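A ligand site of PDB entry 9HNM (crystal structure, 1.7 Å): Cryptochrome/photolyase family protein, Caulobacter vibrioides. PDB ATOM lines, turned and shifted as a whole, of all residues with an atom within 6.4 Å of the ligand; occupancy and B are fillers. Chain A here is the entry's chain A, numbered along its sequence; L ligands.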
ATOM      1  N   ASP A 346      14.949  -0.466  12.558  1.00  0.00           N
ATOM      2  CA  ASP A 346      14.797  -1.399  13.683  1.00  0.00           C
ATOM      3  C   ASP A 346      13.815  -2.533  13.472  1.00  0.00           C
ATOM      4  O   ASP A 346      13.773  -3.401  14.355  1.00  0.00           O
ATOM      5  CB  ASP A 346      14.354  -0.770  15.020  1.00  0.00           C
ATOM      6  CG  ASP A 346      15.220   0.293  15.496  1.00  0.00           C
ATOM      7  OD1 ASP A 346      16.447   0.104  15.295  1.00  0.00           O
ATOM      8  OD2 ASP A 346      14.739   1.241  16.197  1.00  0.00           O
ATOM      9  N   MET A 347      13.002  -2.538  12.411  1.00  0.00           N
ATOM     10  CA  MET A 347      12.192  -3.727  12.145  1.00  0.00           C
ATOM     11  C   MET A 347      13.055  -4.863  11.616  1.00  0.00           C
ATOM     12  O   MET A 347      13.505  -4.832  10.477  1.00  0.00           O
ATOM     13  CB  MET A 347      10.991  -3.438  11.241  1.00  0.00           C
ATOM     14  CG  MET A 347      10.111  -2.282  11.697  1.00  0.00           C
ATOM     15  SD  MET A 347       8.883  -2.040  10.364  1.00  0.00           S
ATOM     16  CE  MET A 347       9.861  -0.940   9.389  1.00  0.00           C
ATOM     17  N   ALA A 348      13.271  -5.893  12.458  1.00  0.00           N
ATOM     18  CA  ALA A 348      14.310  -6.897  12.195  1.00  0.00           C
ATOM     19  C   ALA A 348      14.041  -7.685  10.918  1.00  0.00           C
ATOM     20  O   ALA A 348      14.961  -7.985  10.152  1.00  0.00           O
ATOM     21  CB  ALA A 348      14.393  -7.900  13.360  1.00  0.00           C
ATOM     22  N   CYS A 349      12.782  -8.049  10.704  1.00  0.00           N
ATOM     23  CA  CYS A 349      12.385  -8.764   9.510  1.00  0.00           C
ATOM     24  C   CYS A 349      12.659  -7.944   8.244  1.00  0.00           C
ATOM     25  O   CYS A 349      13.181  -8.481   7.244  1.00  0.00           O
ATOM     26  CB  CYS A 349      10.888  -9.113   9.605  1.00  0.00           C
ATOM     27  SG  CYS A 349       9.785  -7.648   9.985  1.00  0.00           S
ATOM     28  N   VAL A 350      12.270  -6.652   8.246  1.00  0.00           N
ATOM     29  CA  VAL A 350      12.531  -5.825   7.061  1.00  0.00           C
ATOM     30  C   VAL A 350      14.024  -5.677   6.834  1.00  0.00           C
ATOM     31  O   VAL A 350      14.517  -5.820   5.698  1.00  0.00           O
ATOM     32  CB  VAL A 350      11.852  -4.449   7.200  1.00  0.00           C
ATOM     33  CG1 VAL A 350      12.159  -3.572   5.993  1.00  0.00           C
ATOM     34  CG2 VAL A 350      10.333  -4.640   7.394  1.00  0.00           C
ATOM     35  N   VAL A 371       6.674  -9.781   3.988  1.00  0.00           N
ATOM     36  CA  VAL A 371       7.460  -8.802   4.749  1.00  0.00           C
ATOM     37  C   VAL A 371       7.432  -7.471   3.991  1.00  0.00           C
ATOM     38  O   VAL A 371       6.710  -6.542   4.400  1.00  0.00           O
ATOM     39  CB  VAL A 371       8.900  -9.273   5.017  1.00  0.00           C
ATOM     40  CG1 VAL A 371       9.632  -8.200   5.834  1.00  0.00           C
ATOM     41  CG2 VAL A 371       8.905 -10.630   5.833  1.00  0.00           C
ATOM     42  N   SER A 426      -0.677  -8.973  10.085  1.00  0.00           N
ATOM     43  CA  SER A 426      -0.033  -8.324  11.194  1.00  0.00           C
ATOM     44  C   SER A 426       1.288  -9.006  11.535  1.00  0.00           C
ATOM     45  O   SER A 426       1.702 -10.005  10.931  1.00  0.00           O
ATOM     46  CB  SER A 426      -0.975  -8.307  12.401  1.00  0.00           C
ATOM     47  OG  SER A 426      -1.020  -9.640  12.915  1.00  0.00           O
ATOM     48  N   GLY A 427       1.971  -8.484  12.560  1.00  0.00           N
ATOM     49  CA  GLY A 427       3.209  -9.120  13.005  1.00  0.00           C
ATOM     50  C   GLY A 427       3.030 -10.557  13.489  1.00  0.00           C
ATOM     51  O   GLY A 427       3.977 -11.366  13.443  1.00  0.00           O
ATOM     52  N   ALA A 428       1.814 -10.901  13.953  1.00  0.00           N
ATOM     53  CA  ALA A 428       1.568 -12.268  14.412  1.00  0.00           C
ATOM     54  C   ALA A 428       1.924 -13.274  13.339  1.00  0.00           C
ATOM     55  O   ALA A 428       2.410 -14.380  13.640  1.00  0.00           O
ATOM     56  CB  ALA A 428       0.115 -12.422  14.859  1.00  0.00           C
ATOM     57  N   ILE A 430       4.275 -12.945  10.972  1.00  0.00           N
ATOM     58  CA  ILE A 430       5.725 -13.038  10.849  1.00  0.00           C
ATOM     59  C   ILE A 430       6.298 -13.801  12.042  1.00  0.00           C
ATOM     60  O   ILE A 430       7.204 -14.623  11.888  1.00  0.00           O
ATOM     61  CB  ILE A 430       6.319 -11.637  10.709  1.00  0.00           C
ATOM     62  CG1 ILE A 430       5.790 -11.021   9.391  1.00  0.00           C
ATOM     63  CG2 ILE A 430       7.866 -11.728  10.690  1.00  0.00           C
ATOM     64  CD1 ILE A 430       6.077  -9.496   9.255  1.00  0.00           C
ATOM     65  N   ASP A 431       5.749 -13.542  13.238  1.00  0.00           N
ATOM     66  CA  ASP A 431       6.173 -14.287  14.425  1.00  0.00           C
ATOM     67  C   ASP A 431       5.893 -15.771  14.301  1.00  0.00           C
ATOM     68  O   ASP A 431       6.721 -16.599  14.671  1.00  0.00           O
ATOM     69  CB  ASP A 431       5.525 -13.696  15.677  1.00  0.00           C
ATOM     70  CG  ASP A 431       5.991 -14.375  16.927  1.00  0.00           C
ATOM     71  OD1 ASP A 431       7.217 -14.534  17.140  1.00  0.00           O
ATOM     72  OD2 ASP A 431       5.122 -14.617  17.778  1.00  0.00           O
ATOM     73  N   SER A 434       8.608 -17.296  11.524  1.00  0.00           N
ATOM     74  CA  SER A 434      10.025 -16.907  11.497  1.00  0.00           C
ATOM     75  C   SER A 434      10.600 -16.903  12.899  1.00  0.00           C
ATOM     76  O   SER A 434       9.872 -16.919  13.889  1.00  0.00           O
ATOM     77  CB  SER A 434      10.208 -15.504  10.895  1.00  0.00           C
ATOM     78  OG  SER A 434       9.937 -14.508  11.894  1.00  0.00           O
ATOM     79  N   TYR A 436      12.248 -14.084  13.751  1.00  0.00           N
ATOM     80  CA  TYR A 436      12.711 -12.718  13.771  1.00  0.00           C
ATOM     81  C   TYR A 436      12.324 -12.007  15.057  1.00  0.00           C
ATOM     82  O   TYR A 436      13.059 -11.147  15.527  1.00  0.00           O
ATOM     83  CB  TYR A 436      12.116 -11.902  12.622  1.00  0.00           C
ATOM     84  CG  TYR A 436      12.717 -12.136  11.286  1.00  0.00           C
ATOM     85  CD1 TYR A 436      11.922 -12.520  10.215  1.00  0.00           C
ATOM     86  CD2 TYR A 436      14.101 -11.962  11.083  1.00  0.00           C
ATOM     87  CE1 TYR A 436      12.478 -12.728   8.967  1.00  0.00           C
ATOM     88  CE2 TYR A 436      14.660 -12.177   9.799  1.00  0.00           C
ATOM     89  CZ  TYR A 436      13.839 -12.575   8.792  1.00  0.00           C
ATOM     90  OH  TYR A 436      14.367 -12.785   7.561  1.00  0.00           O
ATOM     91  N   CYS A 437      11.134 -12.252  15.573  1.00  0.00           N
ATOM     92  CA  CYS A 437      10.588 -11.311  16.544  1.00  0.00           C
ATOM     93  C   CYS A 437      11.264 -11.396  17.912  1.00  0.00           C
ATOM     94  O   CYS A 437      11.307 -10.388  18.652  1.00  0.00           O
ATOM     95  CB  CYS A 437       9.087 -11.519  16.666  1.00  0.00           C
ATOM     96  SG  CYS A 437       8.179 -11.353  15.111  1.00  0.00           S
ATOM     97  N   LYS A 438      11.808 -12.562  18.281  1.00  0.00           N
ATOM     98  CA  LYS A 438      12.494 -12.643  19.575  1.00  0.00           C
ATOM     99  C   LYS A 438      13.704 -11.724  19.606  1.00  0.00           C
ATOM    100  O   LYS A 438      14.012 -11.124  20.651  1.00  0.00           O
ATOM    101  CB  LYS A 438      12.875 -14.102  19.877  1.00  0.00           C
ATOM    102  CG  LYS A 438      14.128 -14.573  19.106  1.00  0.00           C
ATOM    103  CD  LYS A 438      13.842 -15.778  18.227  1.00  0.00           C
ATOM    104  CE  LYS A 438      13.604 -17.028  19.077  1.00  0.00           C
ATOM    105  NZ  LYS A 438      13.144 -18.195  18.271  1.00  0.00           N
ATOM    106  N   CYS A 440      13.901  -8.836  17.853  1.00  0.00           N
ATOM    107  CA  CYS A 440      13.566  -7.507  17.408  1.00  0.00           C
ATOM    108  C   CYS A 440      13.366  -6.562  18.588  1.00  0.00           C
ATOM    109  O   CYS A 440      12.895  -6.959  19.640  1.00  0.00           O
ATOM    110  CB  CYS A 440      12.269  -7.573  16.607  1.00  0.00           C
ATOM    111  SG  CYS A 440      11.835  -6.073  15.769  1.00  0.00           S
ATOM    112  N   ARG A 441      13.709  -5.282  18.370  1.00  0.00           N
ATOM    113  CA  ARG A 441      13.442  -4.228  19.351  1.00  0.00           C
ATOM    114  C   ARG A 441      11.964  -4.073  19.655  1.00  0.00           C
ATOM    115  O   ARG A 441      11.596  -3.671  20.760  1.00  0.00           O
ATOM    116  CB  ARG A 441      13.963  -2.926  18.789  1.00  0.00           C
ATOM    117  CG  ARG A 441      13.126  -1.781  19.176  1.00  0.00           C
ATOM    118  CD  ARG A 441      13.816  -0.500  18.944  1.00  0.00           C
ATOM    119  NE  ARG A 441      12.849   0.584  18.837  1.00  0.00           N
ATOM    120  CZ  ARG A 441      11.887   0.842  19.716  1.00  0.00           C
ATOM    121  NH1 ARG A 441      11.746   0.158  20.855  1.00  0.00           N
ATOM    122  NH2 ARG A 441      11.083   1.891  19.486  1.00  0.00           N
ATOM    123  N   TYR A 442      11.109  -4.334  18.679  1.00  0.00           N
ATOM    124  CA  TYR A 442       9.679  -4.140  18.861  1.00  0.00           C
ATOM    125  C   TYR A 442       9.040  -5.358  19.525  1.00  0.00           C
ATOM    126  O   TYR A 442       9.559  -6.468  19.468  1.00  0.00           O
ATOM    127  CB  TYR A 442       9.010  -3.856  17.509  1.00  0.00           C
ATOM    128  CG  TYR A 442       9.455  -2.541  16.882  1.00  0.00           C
ATOM    129  CD1 TYR A 442       9.025  -1.308  17.391  1.00  0.00           C
ATOM    130  CD2 TYR A 442      10.272  -2.529  15.752  1.00  0.00           C
ATOM    131  CE1 TYR A 442       9.416  -0.090  16.795  1.00  0.00           C
ATOM    132  CE2 TYR A 442      10.667  -1.323  15.150  1.00  0.00           C
ATOM    133  CZ  TYR A 442      10.227  -0.107  15.670  1.00  0.00           C
ATOM    134  OH  TYR A 442      10.612   1.089  15.063  1.00  0.00           O
ATOM    135  N   ASP A 443       7.920  -5.115  20.217  1.00  0.00           N
ATOM    136  CA  ASP A 443       7.133  -6.165  20.849  1.00  0.00           C
ATOM    137  C   ASP A 443       5.975  -6.549  19.939  1.00  0.00           C
ATOM    138  O   ASP A 443       5.031  -5.772  19.773  1.00  0.00           O
ATOM    139  CB  ASP A 443       6.595  -5.719  22.213  1.00  0.00           C
ATOM    140  CG  ASP A 443       5.967  -6.865  22.993  1.00  0.00           C
ATOM    141  OD1 ASP A 443       5.636  -7.922  22.398  1.00  0.00           O
ATOM    142  OD2 ASP A 443       5.854  -6.749  24.216  1.00  0.00           O
ATOM    143  N   VAL A 444       6.023  -7.762  19.410  1.00  0.00           N
ATOM    144  CA  VAL A 444       4.987  -8.246  18.487  1.00  0.00           C
ATOM    145  C   VAL A 444       3.632  -8.487  19.175  1.00  0.00           C
ATOM    146  O   VAL A 444       2.611  -8.627  18.489  1.00  0.00           O
ATOM    147  CB  VAL A 444       5.507  -9.509  17.756  1.00  0.00           C
ATOM    148  CG1 VAL A 444       5.534 -10.762  18.645  1.00  0.00           C
ATOM    149  CG2 VAL A 444       4.778  -9.725  16.438  1.00  0.00           C
ATOM    150  N   ALA A 452       5.622  -0.953  20.070  1.00  0.00           N
ATOM    151  CA  ALA A 452       4.750  -1.882  19.369  1.00  0.00           C
ATOM    152  C   ALA A 452       5.294  -2.190  17.973  1.00  0.00           C
ATOM    153  O   ALA A 452       5.707  -1.283  17.239  1.00  0.00           O
ATOM    154  CB  ALA A 452       3.345  -1.340  19.236  1.00  0.00           C
ATOM    155  N   CYS A 453       5.225  -3.439  17.617  1.00  0.00           N
ATOM    156  CA  CYS A 453       5.501  -3.848  16.228  1.00  0.00           C
ATOM    157  C   CYS A 453       4.684  -3.018  15.242  1.00  0.00           C
ATOM    158  O   CYS A 453       3.435  -3.073  15.285  1.00  0.00           O
ATOM    159  CB  CYS A 453       5.159  -5.323  16.038  1.00  0.00           C
ATOM    160  SG  CYS A 453       5.225  -5.883  14.296  1.00  0.00           S
ATOM    161  N   PRO A 454       5.328  -2.302  14.295  1.00  0.00           N
ATOM    162  CA  PRO A 454       4.551  -1.422  13.389  1.00  0.00           C
ATOM    163  C   PRO A 454       3.544  -2.145  12.547  1.00  0.00           C
ATOM    164  O   PRO A 454       2.536  -1.543  12.166  1.00  0.00           O
ATOM    165  CB  PRO A 454       5.631  -0.736  12.523  1.00  0.00           C
ATOM    166  CG  PRO A 454       6.878  -0.802  13.397  1.00  0.00           C
ATOM    167  CD  PRO A 454       6.787  -2.092  14.192  1.00  0.00           C
ATOM    168  N   PHE A 455       3.768  -3.436  12.226  1.00  0.00           N
ATOM    169  CA  PHE A 455       2.804  -4.172  11.410  1.00  0.00           C
ATOM    170  C   PHE A 455       1.429  -4.257  12.081  1.00  0.00           C
ATOM    171  O   PHE A 455       0.409  -4.421  11.377  1.00  0.00           O
ATOM    172  CB  PHE A 455       3.267  -5.583  11.137  1.00  0.00           C
ATOM    173  CG  PHE A 455       4.345  -5.710  10.091  1.00  0.00           C
ATOM    174  CD1 PHE A 455       5.690  -5.607  10.440  1.00  0.00           C
ATOM    175  CD2 PHE A 455       4.009  -5.889   8.783  1.00  0.00           C
ATOM    176  CE1 PHE A 455       6.712  -5.751   9.462  1.00  0.00           C
ATOM    177  CE2 PHE A 455       5.037  -6.028   7.782  1.00  0.00           C
ATOM    178  CZ  PHE A 455       6.361  -5.954   8.124  1.00  0.00           C
ATOM    179  N   ASN A 456       1.370  -4.211  13.425  1.00  0.00           N
ATOM    180  CA  ASN A 456       0.107  -4.485  14.093  1.00  0.00           C
ATOM    181  C   ASN A 456      -0.901  -3.324  13.913  1.00  0.00           C
ATOM    182  O   ASN A 456      -2.034  -3.557  13.488  1.00  0.00           O
ATOM    183  CB  ASN A 456       0.344  -4.778  15.595  1.00  0.00           C
ATOM    184  CG  ASN A 456       1.068  -6.117  15.797  1.00  0.00           C
ATOM    185  OD1 ASN A 456       1.055  -6.968  14.932  1.00  0.00           O
ATOM    186  ND2 ASN A 456       1.629  -6.314  16.953  1.00  0.00           N
HETATM  187 FE1  LIG L   1       8.558  -9.217  14.367  1.00  0.00          FE
HETATM  188 FE2  LIG L   1       7.358  -6.789  14.104  1.00  0.00          FE
HETATM  189 FE3  LIG L   1       9.156  -7.689  12.167  1.00  0.00          FE
HETATM  190 FE4  LIG L   1      10.016  -6.883  14.668  1.00  0.00          FE
HETATM  191  S1  LIG L   1       9.030  -5.568  13.122  1.00  0.00           S
HETATM  192  S2  LIG L   1      10.607  -8.777  13.486  1.00  0.00           S
HETATM  193  S3  LIG L   1       8.299  -7.600  15.953  1.00  0.00           S
HETATM  194  S4  LIG L   1       7.163  -8.602  12.703  1.00  0.00           S
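A sulfur (S2) of the ligand sits close to the backbone NH (N) of Cys 349, 3.6 Å away.
FE3 of the ligand is bound by SG of Cys 349, 2.3 Å away.
SG of Cys 440 is bound to FE4 of the ligand, 2.3 Å away.
The side-chain sulfur (SG) of Cys 437 binds an iron atom (FE1) of the ligand (2.3 Å).
FE2 of the ligand is bound by SG of Cys 453, 2.3 Å away.
SG of Cys 440 sits close to N of Ala 348.
The backbone carbonyl oxygen (O) of Asp 346 sits close to the side-chain sulfur (SG) of Cys 440, at 3.6 Å.
The side-chain sulfur of Cys 437 sits close to the backbone NH of Asp 431 (3.8 Å).
The side-chain sulfur (SG) of Cys 453 sits close to the backbone NH (N) of Phe 455.
The backbone NH of Cys 453 sits at hydrogen-bond distance from the backbone carbonyl oxygen of Asp 443.
N of Tyr 436 is in hydrogen-bond range of OG of Ser 434 (3.0 Å).
The side-chain hydroxyl (OG) of Ser 434 lies within hydrogen-bond range of the backbone carbonyl oxygen (O) of Ile 430 (2.7 Å).
The backbone NH (N) of Gly 427 lies within hydrogen-bond range of the side-chain amide oxygen (OD1) of Asn 456, 3.0 Å away.
Residues that only touch the ligand: Met 347 (3.5 Å), Tyr 436 (3.6 Å), Ile 430 (3.7 Å), Val 444 (3.8 Å), Ala 348 (3.9 Å), Tyr 442 (3.9 Å) and Gly 427 (3.999 Å).
Of the 25 residues printed, 11 come within 4 Å of the ligand.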
